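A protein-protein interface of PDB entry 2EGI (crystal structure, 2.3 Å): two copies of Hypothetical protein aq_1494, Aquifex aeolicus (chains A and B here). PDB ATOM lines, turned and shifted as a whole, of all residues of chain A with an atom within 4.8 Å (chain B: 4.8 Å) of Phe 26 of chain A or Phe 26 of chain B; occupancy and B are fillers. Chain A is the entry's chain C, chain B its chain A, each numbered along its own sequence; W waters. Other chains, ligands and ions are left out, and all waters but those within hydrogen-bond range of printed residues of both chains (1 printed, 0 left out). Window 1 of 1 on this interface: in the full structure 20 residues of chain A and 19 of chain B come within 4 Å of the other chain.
Phe 26 of chain A touches just these residues of chain B: His 22 (3.9 Å) and Phe 26 (3.3 Å).
Of the printed residues of chain A, Phe 26 of chain B touches His 22 and Phe 26.
Printed residues of chain B within 4 Å of Ala 59 of chain A: Tyr 60 and Cys 61.
Of the printed residues of chain A, Asn 24 of chain B touches Arg 27 (3.0 Å).
Printed residues of chain B within 4 Å of Cys 61 of chain A: Ala 59.
Of the printed residues of chain A, Glu 30 of chain B touches His 22 (3.8 Å).
Of the printed residues of chain B, Ser 23 of chain A touches Ser 23 and Arg 27.
The nearest residue of chain A that does not touch Phe 26 of chain B is Ser 23 of chain A (4.3 Å).
The nearest printed residue of chain B that does not touch Glu 30 of chain A is Ser 23 of chain B (7.0 Å).
NE of Arg 27 of chain B is in hydrogen-bond range of OG of Ser 23 of chain A (2.9 Å).
The guanidinium group (NE) of Arg 27 of chain A sits at hydrogen-bond distance from the side-chain hydroxyl (OG) of Ser 23 of chain B.
The backbone NH of Ala 59 of chain A sits at hydrogen-bond distance from the backbone carbonyl oxygen of Cys 61 of chain B, at 3.1 Å.
The guanidinium group (NH2) of Arg 27 of chain A sits close to the guanidinium group (NH2) of Arg 27 of chain B (3.4 Å).
The side-chain amide nitrogen (ND2) of Asn 24 of chain B lies close to the guanidinium group (NH2) of Arg 27 of chain A (3.0 Å).
The guanidinium group of Arg 27 of chain B lies within hydrogen-bond range of the side-chain amide oxygen of Asn 24 of chain A (2.9 Å).
N of Ala 59 of chain B is in hydrogen-bond range of O of Cys 61 of chain A.
His 22 of chain A touches Phe 26 of chain B, and with the chains exchanged Phe 26 of chain A touches His 22 of chain B.
Ser 23 of chain A touches Arg 27 of chain B, and with the chains exchanged Arg 27 of chain A touches Ser 23 of chain B.
Asn 24 of chain A touches Arg 27 of chain B, and with the chains exchanged Arg 27 of chain A touches Asn 24 of chain B.
Ala 59 of chain A touches Cys 61 of chain B, and with the chains exchanged Cys 61 of chain A touches Ala 59 of chain B.
Positions printed for both chains: 22, 23, 24, 25, 26, 27, 28, 29, 30, 59, 60, 61 and 63.
Of the 15 pairs that touch across the chains among the printed residues, 15 have their exchanged pair printed and touching as well.
His 22 of chain A touches Phe 26 of chain B (NE2 to CB, 3.9 Å).
CE1 of His 22 of chain A touches OE1 of Glu 30 of chain B (3.8 Å).
CB of Ser 23 of chain A touches O of Ser 23 of chain B (3.5 Å).
Phe 26 of chain A touches His 22 of chain B (CB to CE1, 3.9 Å).
Phe 26 of chain A touches Phe 26 of chain B.
Glu 30 of chain A touches His 22 of chain B (OE2 to NE2, 3.9 Å).
O of Ala 59 of chain A touches CA of Tyr 60 of chain B, 3.5 Å away.
Ala 59 of chain B touches Tyr 60 of chain A (O to CA, 3.4 Å).
Hydrophobic or aromatic side chains of chain A that line the printed part of chain B: His 22, Phe 26 and Tyr 60.
Among the printed residues, 15 pairs touch across the chains.
Among the printed residues, no Asp or Glu carboxylate lies within 4 Å of a Lys or Arg side-chain nitrogen of the other chain.
The side-chain hydroxyl (OH) of Tyr 63 of chain B sits close to the side-chain sulfur (SG) of Cys 61 of chain B, 3.7 Å away.
OH of Tyr 63 of chain A is in hydrogen-bond range of O of His 22 of chain A.
The backbone carbonyl oxygen of His 22 of chain B lies within hydrogen-bond range of the side-chain hydroxyl of Tyr 63 of chain B (2.9 Å).
SG of Cys 61 of chain A lies close to OH of Tyr 63 of chain A, 3.8 Å away.
Water W1 bridges a ring nitrogen (NE2) of His 22 of chain A (2.7 Å) and the backbone carbonyl oxygen (O) of Phe 26 of chain B (2.7 Å).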
ATOM      1  N   HIS A  22     -16.564 -14.395 -18.140  1.00  0.00           N
ATOM      2  CA  HIS A  22     -16.036 -14.159 -16.801  1.00  0.00           C
ATOM      3  C   HIS A  22     -16.089 -15.334 -15.827  1.00  0.00           C
ATOM      4  O   HIS A  22     -15.204 -15.479 -15.000  1.00  0.00           O
ATOM      5  CB  HIS A  22     -16.697 -12.928 -16.165  1.00  0.00           C
ATOM      6  CG  HIS A  22     -18.157 -13.081 -15.872  1.00  0.00           C
ATOM      7  ND1 HIS A  22     -19.131 -12.947 -16.838  1.00  0.00           N
ATOM      8  CD2 HIS A  22     -18.816 -13.256 -14.699  1.00  0.00           C
ATOM      9  CE1 HIS A  22     -20.324 -13.022 -16.272  1.00  0.00           C
ATOM     10  NE2 HIS A  22     -20.161 -13.208 -14.975  1.00  0.00           N
ATOM     11  N   SER A  23     -17.119 -16.170 -15.932  1.00  0.00           N
ATOM     12  CA  SER A  23     -17.280 -17.316 -15.042  1.00  0.00           C
ATOM     13  C   SER A  23     -16.205 -18.389 -15.210  1.00  0.00           C
ATOM     14  O   SER A  23     -15.923 -19.141 -14.283  1.00  0.00           O
ATOM     15  CB  SER A  23     -18.650 -17.953 -15.257  1.00  0.00           C
ATOM     16  OG  SER A  23     -18.747 -18.486 -16.566  1.00  0.00           O
ATOM     17  N   ASN A  24     -15.610 -18.480 -16.388  1.00  0.00           N
ATOM     18  CA  ASN A  24     -14.592 -19.496 -16.589  1.00  0.00           C
ATOM     19  C   ASN A  24     -13.282 -19.201 -15.850  1.00  0.00           C
ATOM     20  O   ASN A  24     -12.517 -20.111 -15.543  1.00  0.00           O
ATOM     21  CB  ASN A  24     -14.354 -19.703 -18.085  1.00  0.00           C
ATOM     22  CG  ASN A  24     -15.539 -20.369 -18.766  1.00  0.00           C
ATOM     23  OD1 ASN A  24     -16.168 -21.261 -18.196  1.00  0.00           O
ATOM     24  ND2 ASN A  24     -15.841 -19.948 -19.989  1.00  0.00           N
ATOM     25  N   TYR A  25     -13.031 -17.932 -15.548  1.00  0.00           N
ATOM     26  CA  TYR A  25     -11.820 -17.566 -14.825  1.00  0.00           C
ATOM     27  C   TYR A  25     -11.718 -18.373 -13.527  1.00  0.00           C
ATOM     28  O   TYR A  25     -10.649 -18.876 -13.179  1.00  0.00           O
ATOM     29  CB  TYR A  25     -11.823 -16.063 -14.524  1.00  0.00           C
ATOM     30  CG  TYR A  25     -11.466 -15.210 -15.724  1.00  0.00           C
ATOM     31  CD1 TYR A  25     -10.198 -14.639 -15.841  1.00  0.00           C
ATOM     32  CD2 TYR A  25     -12.380 -15.005 -16.760  1.00  0.00           C
ATOM     33  CE1 TYR A  25      -9.848 -13.883 -16.962  1.00  0.00           C
ATOM     34  CE2 TYR A  25     -12.042 -14.256 -17.889  1.00  0.00           C
ATOM     35  CZ  TYR A  25     -10.772 -13.694 -17.981  1.00  0.00           C
ATOM     36  OH  TYR A  25     -10.433 -12.924 -19.064  1.00  0.00           O
ATOM     37  N   PHE A  26     -12.834 -18.505 -12.819  1.00  0.00           N
ATOM     38  CA  PHE A  26     -12.836 -19.254 -11.574  1.00  0.00           C
ATOM     39  C   PHE A  26     -12.484 -20.715 -11.859  1.00  0.00           C
ATOM     40  O   PHE A  26     -11.905 -21.400 -11.016  1.00  0.00           O
ATOM     41  CB  PHE A  26     -14.202 -19.132 -10.882  1.00  0.00           C
ATOM     42  CG  PHE A  26     -14.512 -17.732 -10.408  1.00  0.00           C
ATOM     43  CD1 PHE A  26     -13.960 -17.242  -9.226  1.00  0.00           C
ATOM     44  CD2 PHE A  26     -15.301 -16.877 -11.186  1.00  0.00           C
ATOM     45  CE1 PHE A  26     -14.181 -15.917  -8.821  1.00  0.00           C
ATOM     46  CE2 PHE A  26     -15.531 -15.552 -10.800  1.00  0.00           C
ATOM     47  CZ  PHE A  26     -14.968 -15.067  -9.610  1.00  0.00           C
ATOM     48  N   ARG A  27     -12.816 -21.188 -13.054  1.00  0.00           N
ATOM     49  CA  ARG A  27     -12.498 -22.562 -13.414  1.00  0.00           C
ATOM     50  C   ARG A  27     -10.984 -22.654 -13.640  1.00  0.00           C
ATOM     51  O   ARG A  27     -10.352 -23.644 -13.272  1.00  0.00           O
ATOM     52  CB  ARG A  27     -13.299 -22.981 -14.652  1.00  0.00           C
ATOM     53  CG  ARG A  27     -14.796 -22.823 -14.437  1.00  0.00           C
ATOM     54  CD  ARG A  27     -15.628 -23.493 -15.518  1.00  0.00           C
ATOM     55  NE  ARG A  27     -17.057 -23.407 -15.222  1.00  0.00           N
ATOM     56  CZ  ARG A  27     -18.010 -24.001 -15.937  1.00  0.00           C
ATOM     57  NH1 ARG A  27     -17.692 -24.726 -17.002  1.00  0.00           N
ATOM     58  NH2 ARG A  27     -19.283 -23.890 -15.579  1.00  0.00           N
ATOM     59  N   TYR A  28     -10.405 -21.603 -14.216  1.00  0.00           N
ATOM     60  CA  TYR A  28      -8.962 -21.554 -14.435  1.00  0.00           C
ATOM     61  C   TYR A  28      -8.255 -21.560 -13.077  1.00  0.00           C
ATOM     62  O   TYR A  28      -7.243 -22.245 -12.898  1.00  0.00           O
ATOM     63  CB  TYR A  28      -8.544 -20.283 -15.193  1.00  0.00           C
ATOM     64  CG  TYR A  28      -9.055 -20.187 -16.616  1.00  0.00           C
ATOM     65  CD1 TYR A  28      -9.312 -21.336 -17.367  1.00  0.00           C
ATOM     66  CD2 TYR A  28      -9.251 -18.947 -17.226  1.00  0.00           C
ATOM     67  CE1 TYR A  28      -9.754 -21.254 -18.691  1.00  0.00           C
ATOM     68  CE2 TYR A  28      -9.693 -18.855 -18.562  1.00  0.00           C
ATOM     69  CZ  TYR A  28      -9.941 -20.013 -19.282  1.00  0.00           C
ATOM     70  OH  TYR A  28     -10.366 -19.936 -20.586  1.00  0.00           O
ATOM     71  N   PHE A  29      -8.783 -20.802 -12.119  1.00  0.00           N
ATOM     72  CA  PHE A  29      -8.145 -20.755 -10.807  1.00  0.00           C
ATOM     73  C   PHE A  29      -8.243 -22.116 -10.117  1.00  0.00           C
ATOM     74  O   PHE A  29      -7.347 -22.505  -9.363  1.00  0.00           O
ATOM     75  CB  PHE A  29      -8.765 -19.667  -9.916  1.00  0.00           C
ATOM     76  CG  PHE A  29      -8.866 -18.307 -10.578  1.00  0.00           C
ATOM     77  CD1 PHE A  29      -7.832 -17.818 -11.378  1.00  0.00           C
ATOM     78  CD2 PHE A  29     -10.004 -17.517 -10.398  1.00  0.00           C
ATOM     79  CE1 PHE A  29      -7.932 -16.561 -11.991  1.00  0.00           C
ATOM     80  CE2 PHE A  29     -10.114 -16.254 -11.008  1.00  0.00           C
ATOM     81  CZ  PHE A  29      -9.080 -15.777 -11.806  1.00  0.00           C
ATOM     82  N   GLU A  30      -9.324 -22.842 -10.380  1.00  0.00           N
ATOM     83  CA  GLU A  30      -9.498 -24.151  -9.768  1.00  0.00           C
ATOM     84  C   GLU A  30      -8.449 -25.107 -10.325  1.00  0.00           C
ATOM     85  O   GLU A  30      -7.907 -25.929  -9.590  1.00  0.00           O
ATOM     86  CB  GLU A  30     -10.897 -24.724 -10.036  1.00  0.00           C
ATOM     87  CG  GLU A  30     -11.179 -26.021  -9.255  1.00  0.00           C
ATOM     88  CD  GLU A  30     -12.453 -26.733  -9.703  1.00  0.00           C
ATOM     89  OE1 GLU A  30     -12.385 -27.588 -10.627  1.00  0.00           O
ATOM     90  OE2 GLU A  30     -13.520 -26.425  -9.134  1.00  0.00           O
ATOM     91  N   ALA A  59     -15.137 -15.832  -3.331  1.00  0.00           N
ATOM     92  CA  ALA A  59     -14.181 -15.644  -4.418  1.00  0.00           C
ATOM     93  C   ALA A  59     -14.426 -14.314  -5.087  1.00  0.00           C
ATOM     94  O   ALA A  59     -15.574 -13.896  -5.268  1.00  0.00           O
ATOM     95  CB  ALA A  59     -14.319 -16.770  -5.450  1.00  0.00           C
ATOM     96  N   TYR A  60     -13.338 -13.656  -5.461  1.00  0.00           N
ATOM     97  CA  TYR A  60     -13.405 -12.357  -6.112  1.00  0.00           C
ATOM     98  C   TYR A  60     -12.536 -12.360  -7.357  1.00  0.00           C
ATOM     99  O   TYR A  60     -11.517 -13.044  -7.404  1.00  0.00           O
ATOM    100  CB  TYR A  60     -12.896 -11.287  -5.151  1.00  0.00           C
ATOM    101  CG  TYR A  60     -12.723  -9.916  -5.757  1.00  0.00           C
ATOM    102  CD1 TYR A  60     -13.807  -9.047  -5.897  1.00  0.00           C
ATOM    103  CD2 TYR A  60     -11.463  -9.470  -6.158  1.00  0.00           C
ATOM    104  CE1 TYR A  60     -13.637  -7.751  -6.418  1.00  0.00           C
ATOM    105  CE2 TYR A  60     -11.277  -8.178  -6.681  1.00  0.00           C
ATOM    106  CZ  TYR A  60     -12.370  -7.326  -6.807  1.00  0.00           C
ATOM    107  OH  TYR A  60     -12.190  -6.063  -7.329  1.00  0.00           O
ATOM    108  N   CYS A  61     -12.940 -11.599  -8.366  1.00  0.00           N
ATOM    109  CA  CYS A  61     -12.145 -11.486  -9.576  1.00  0.00           C
ATOM    110  C   CYS A  61     -12.319 -10.108 -10.199  1.00  0.00           C
ATOM    111  O   CYS A  61     -13.441  -9.613 -10.376  1.00  0.00           O
ATOM    112  CB  CYS A  61     -12.502 -12.561 -10.600  1.00  0.00           C
ATOM    113  SG  CYS A  61     -11.319 -12.606 -11.972  1.00  0.00           S
ATOM    114  N   TYR A  63     -11.505  -7.894 -13.473  1.00  0.00           N
ATOM    115  CA  TYR A  63     -11.211  -8.048 -14.891  1.00  0.00           C
ATOM    116  C   TYR A  63     -10.624  -6.777 -15.505  1.00  0.00           C
ATOM    117  O   TYR A  63     -11.297  -5.756 -15.599  1.00  0.00           O
ATOM    118  CB  TYR A  63     -12.491  -8.470 -15.606  1.00  0.00           C
ATOM    119  CG  TYR A  63     -13.080  -9.738 -15.037  1.00  0.00           C
ATOM    120  CD1 TYR A  63     -12.887 -10.967 -15.666  1.00  0.00           C
ATOM    121  CD2 TYR A  63     -13.816  -9.710 -13.855  1.00  0.00           C
ATOM    122  CE1 TYR A  63     -13.419 -12.140 -15.130  1.00  0.00           C
ATOM    123  CE2 TYR A  63     -14.349 -10.860 -13.313  1.00  0.00           C
ATOM    124  CZ  TYR A  63     -14.154 -12.077 -13.953  1.00  0.00           C
ATOM    125  OH  TYR A  63     -14.733 -13.213 -13.434  1.00  0.00           O
ATOM    126  N   HIS B  22     -19.352 -23.461  -7.867  1.00  0.00           N
ATOM    127  CA  HIS B  22     -19.328 -22.037  -7.543  1.00  0.00           C
ATOM    128  C   HIS B  22     -19.309 -21.100  -8.749  1.00  0.00           C
ATOM    129  O   HIS B  22     -19.901 -20.027  -8.701  1.00  0.00           O
ATOM    130  CB  HIS B  22     -18.152 -21.729  -6.604  1.00  0.00           C
ATOM    131  CG  HIS B  22     -16.814 -22.132  -7.143  1.00  0.00           C
ATOM    132  ND1 HIS B  22     -15.983 -21.257  -7.811  1.00  0.00           N
ATOM    133  CD2 HIS B  22     -16.150 -23.311  -7.085  1.00  0.00           C
ATOM    134  CE1 HIS B  22     -14.862 -21.876  -8.136  1.00  0.00           C
ATOM    135  NE2 HIS B  22     -14.940 -23.123  -7.707  1.00  0.00           N
ATOM    136  N   SER B  23     -18.644 -21.511  -9.828  1.00  0.00           N
ATOM    137  CA  SER B  23     -18.558 -20.697 -11.042  1.00  0.00           C
ATOM    138  C   SER B  23     -19.905 -20.504 -11.732  1.00  0.00           C
ATOM    139  O   SER B  23     -20.082 -19.541 -12.485  1.00  0.00           O
ATOM    140  CB  SER B  23     -17.580 -21.323 -12.045  1.00  0.00           C
ATOM    141  OG  SER B  23     -18.114 -22.509 -12.615  1.00  0.00           O
ATOM    142  N   ASN B  24     -20.846 -21.418 -11.496  1.00  0.00           N
ATOM    143  CA  ASN B  24     -22.168 -21.313 -12.122  1.00  0.00           C
ATOM    144  C   ASN B  24     -23.054 -20.233 -11.496  1.00  0.00           C
ATOM    145  O   ASN B  24     -24.017 -19.771 -12.117  1.00  0.00           O
ATOM    146  CB  ASN B  24     -22.890 -22.664 -12.091  1.00  0.00           C
ATOM    147  CG  ASN B  24     -22.335 -23.652 -13.114  1.00  0.00           C
ATOM    148  OD1 ASN B  24     -22.395 -24.860 -12.913  1.00  0.00           O
ATOM    149  ND2 ASN B  24     -21.808 -23.142 -14.213  1.00  0.00           N
ATOM    150  N   TYR B  25     -22.740 -19.824 -10.273  1.00  0.00           N
ATOM    151  CA  TYR B  25     -23.521 -18.770  -9.614  1.00  0.00           C
ATOM    152  C   TYR B  25     -23.434 -17.474 -10.433  1.00  0.00           C
ATOM    153  O   TYR B  25     -24.415 -16.767 -10.603  1.00  0.00           O
ATOM    154  CB  TYR B  25     -23.002 -18.536  -8.194  1.00  0.00           C
ATOM    155  CG  TYR B  25     -23.441 -19.593  -7.214  1.00  0.00           C
ATOM    156  CD1 TYR B  25     -24.449 -19.333  -6.286  1.00  0.00           C
ATOM    157  CD2 TYR B  25     -22.878 -20.870  -7.239  1.00  0.00           C
ATOM    158  CE1 TYR B  25     -24.889 -20.320  -5.409  1.00  0.00           C
ATOM    159  CE2 TYR B  25     -23.312 -21.861  -6.366  1.00  0.00           C
ATOM    160  CZ  TYR B  25     -24.313 -21.580  -5.456  1.00  0.00           C
ATOM    161  OH  TYR B  25     -24.728 -22.549  -4.577  1.00  0.00           O
ATOM    162  N   PHE B  26     -22.251 -17.177 -10.954  1.00  0.00           N
ATOM    163  CA  PHE B  26     -22.074 -15.980 -11.764  1.00  0.00           C
ATOM    164  C   PHE B  26     -22.952 -16.061 -13.007  1.00  0.00           C
ATOM    165  O   PHE B  26     -23.405 -15.044 -13.542  1.00  0.00           O
ATOM    166  CB  PHE B  26     -20.596 -15.835 -12.116  1.00  0.00           C
ATOM    167  CG  PHE B  26     -19.725 -15.660 -10.902  1.00  0.00           C
ATOM    168  CD1 PHE B  26     -19.736 -14.460 -10.196  1.00  0.00           C
ATOM    169  CD2 PHE B  26     -18.979 -16.725 -10.402  1.00  0.00           C
ATOM    170  CE1 PHE B  26     -19.024 -14.322  -9.004  1.00  0.00           C
ATOM    171  CE2 PHE B  26     -18.264 -16.600  -9.208  1.00  0.00           C
ATOM    172  CZ  PHE B  26     -18.291 -15.394  -8.509  1.00  0.00           C
ATOM    173  N   ARG B  27     -23.206 -17.282 -13.460  1.00  0.00           N
ATOM    174  CA  ARG B  27     -24.055 -17.459 -14.620  1.00  0.00           C
ATOM    175  C   ARG B  27     -25.501 -17.203 -14.188  1.00  0.00           C
ATOM    176  O   ARG B  27     -26.291 -16.663 -14.958  1.00  0.00           O
ATOM    177  CB  ARG B  27     -23.861 -18.859 -15.202  1.00  0.00           C
ATOM    178  CG  ARG B  27     -22.441 -19.065 -15.730  1.00  0.00           C
ATOM    179  CD  ARG B  27     -22.230 -20.390 -16.437  1.00  0.00           C
ATOM    180  NE  ARG B  27     -20.826 -20.542 -16.845  1.00  0.00           N
ATOM    181  CZ  ARG B  27     -20.382 -21.472 -17.691  1.00  0.00           C
ATOM    182  NH1 ARG B  27     -21.228 -22.348 -18.231  1.00  0.00           N
ATOM    183  NH2 ARG B  27     -19.094 -21.527 -18.002  1.00  0.00           N
ATOM    184  N   TYR B  28     -25.833 -17.571 -12.950  1.00  0.00           N
ATOM    185  CA  TYR B  28     -27.178 -17.341 -12.421  1.00  0.00           C
ATOM    186  C   TYR B  28     -27.408 -15.835 -12.289  1.00  0.00           C
ATOM    187  O   TYR B  28     -28.513 -15.350 -12.538  1.00  0.00           O
ATOM    188  CB  TYR B  28     -27.367 -17.982 -11.036  1.00  0.00           C
ATOM    189  CG  TYR B  28     -27.325 -19.498 -10.987  1.00  0.00           C
ATOM    190  CD1 TYR B  28     -27.668 -20.277 -12.097  1.00  0.00           C
ATOM    191  CD2 TYR B  28     -27.005 -20.155  -9.803  1.00  0.00           C
ATOM    192  CE1 TYR B  28     -27.692 -21.675 -12.015  1.00  0.00           C
ATOM    193  CE2 TYR B  28     -27.032 -21.537  -9.711  1.00  0.00           C
ATOM    194  CZ  TYR B  28     -27.378 -22.297 -10.812  1.00  0.00           C
ATOM    195  OH  TYR B  28     -27.441 -23.667 -10.684  1.00  0.00           O
ATOM    196  N   PHE B  29     -26.368 -15.107 -11.880  1.00  0.00           N
ATOM    197  CA  PHE B  29     -26.460 -13.655 -11.737  1.00  0.00           C
ATOM    198  C   PHE B  29     -26.604 -13.009 -13.113  1.00  0.00           C
ATOM    199  O   PHE B  29     -27.258 -11.982 -13.258  1.00  0.00           O
ATOM    200  CB  PHE B  29     -25.219 -13.072 -11.042  1.00  0.00           C
ATOM    201  CG  PHE B  29     -24.871 -13.744  -9.735  1.00  0.00           C
ATOM    202  CD1 PHE B  29     -25.869 -14.150  -8.854  1.00  0.00           C
ATOM    203  CD2 PHE B  29     -23.540 -13.954  -9.384  1.00  0.00           C
ATOM    204  CE1 PHE B  29     -25.543 -14.749  -7.647  1.00  0.00           C
ATOM    205  CE2 PHE B  29     -23.199 -14.553  -8.182  1.00  0.00           C
ATOM    206  CZ  PHE B  29     -24.201 -14.955  -7.309  1.00  0.00           C
ATOM    207  N   GLU B  30     -25.993 -13.609 -14.126  1.00  0.00           N
ATOM    208  CA  GLU B  30     -26.106 -13.054 -15.468  1.00  0.00           C
ATOM    209  C   GLU B  30     -27.549 -13.203 -15.921  1.00  0.00           C
ATOM    210  O   GLU B  30     -28.121 -12.269 -16.486  1.00  0.00           O
ATOM    211  CB  GLU B  30     -25.164 -13.765 -16.450  1.00  0.00           C
ATOM    212  CG  GLU B  30     -25.224 -13.214 -17.881  1.00  0.00           C
ATOM    213  CD  GLU B  30     -24.260 -13.926 -18.821  1.00  0.00           C
ATOM    214  OE1 GLU B  30     -23.057 -13.584 -18.818  1.00  0.00           O
ATOM    215  OE2 GLU B  30     -24.709 -14.839 -19.550  1.00  0.00           O
ATOM    216  N   ALA B  59     -16.386  -9.066  -9.916  1.00  0.00           N
ATOM    217  CA  ALA B  59     -17.464  -9.904  -9.415  1.00  0.00           C
ATOM    218  C   ALA B  59     -17.072 -10.518  -8.082  1.00  0.00           C
ATOM    219  O   ALA B  59     -15.923 -10.878  -7.883  1.00  0.00           O
ATOM    220  CB  ALA B  59     -17.768 -11.023 -10.435  1.00  0.00           C
ATOM    221  N   TYR B  60     -18.034 -10.642  -7.176  1.00  0.00           N
ATOM    222  CA  TYR B  60     -17.782 -11.230  -5.870  1.00  0.00           C
ATOM    223  C   TYR B  60     -18.929 -12.125  -5.426  1.00  0.00           C
ATOM    224  O   TYR B  60     -20.090 -11.833  -5.701  1.00  0.00           O
ATOM    225  CB  TYR B  60     -17.591 -10.141  -4.823  1.00  0.00           C
ATOM    226  CG  TYR B  60     -17.482 -10.670  -3.400  1.00  0.00           C
ATOM    227  CD1 TYR B  60     -16.260 -11.125  -2.885  1.00  0.00           C
ATOM    228  CD2 TYR B  60     -18.597 -10.680  -2.558  1.00  0.00           C
ATOM    229  CE1 TYR B  60     -16.156 -11.564  -1.560  1.00  0.00           C
ATOM    230  CE2 TYR B  60     -18.507 -11.113  -1.243  1.00  0.00           C
ATOM    231  CZ  TYR B  60     -17.287 -11.549  -0.745  1.00  0.00           C
ATOM    232  OH  TYR B  60     -17.206 -11.927   0.574  1.00  0.00           O
ATOM    233  N   CYS B  61     -18.604 -13.209  -4.729  1.00  0.00           N
ATOM    234  CA  CYS B  61     -19.635 -14.105  -4.229  1.00  0.00           C
ATOM    235  C   CYS B  61     -19.212 -14.800  -2.936  1.00  0.00           C
ATOM    236  O   CYS B  61     -18.100 -15.305  -2.828  1.00  0.00           O
ATOM    237  CB  CYS B  61     -19.995 -15.158  -5.284  1.00  0.00           C
ATOM    238  SG  CYS B  61     -21.522 -16.100  -4.904  1.00  0.00           S
ATOM    239  N   TYR B  63     -20.286 -17.832  -0.327  1.00  0.00           N
ATOM    240  CA  TYR B  63     -21.095 -19.046  -0.336  1.00  0.00           C
ATOM    241  C   TYR B  63     -21.351 -19.499   1.112  1.00  0.00           C
ATOM    242  O   TYR B  63     -20.422 -19.807   1.844  1.00  0.00           O
ATOM    243  CB  TYR B  63     -20.368 -20.129  -1.146  1.00  0.00           C
ATOM    244  CG  TYR B  63     -20.013 -19.694  -2.567  1.00  0.00           C
ATOM    245  CD1 TYR B  63     -20.811 -20.052  -3.655  1.00  0.00           C
ATOM    246  CD2 TYR B  63     -18.900 -18.885  -2.812  1.00  0.00           C
ATOM    247  CE1 TYR B  63     -20.508 -19.609  -4.956  1.00  0.00           C
ATOM    248  CE2 TYR B  63     -18.588 -18.434  -4.105  1.00  0.00           C
ATOM    249  CZ  TYR B  63     -19.390 -18.796  -5.168  1.00  0.00           C
ATOM    250  OH  TYR B  63     -19.084 -18.345  -6.438  1.00  0.00           O
HETATM  251  O   HOH W   1     -22.297 -12.563 -13.489  1.00  0.00           O
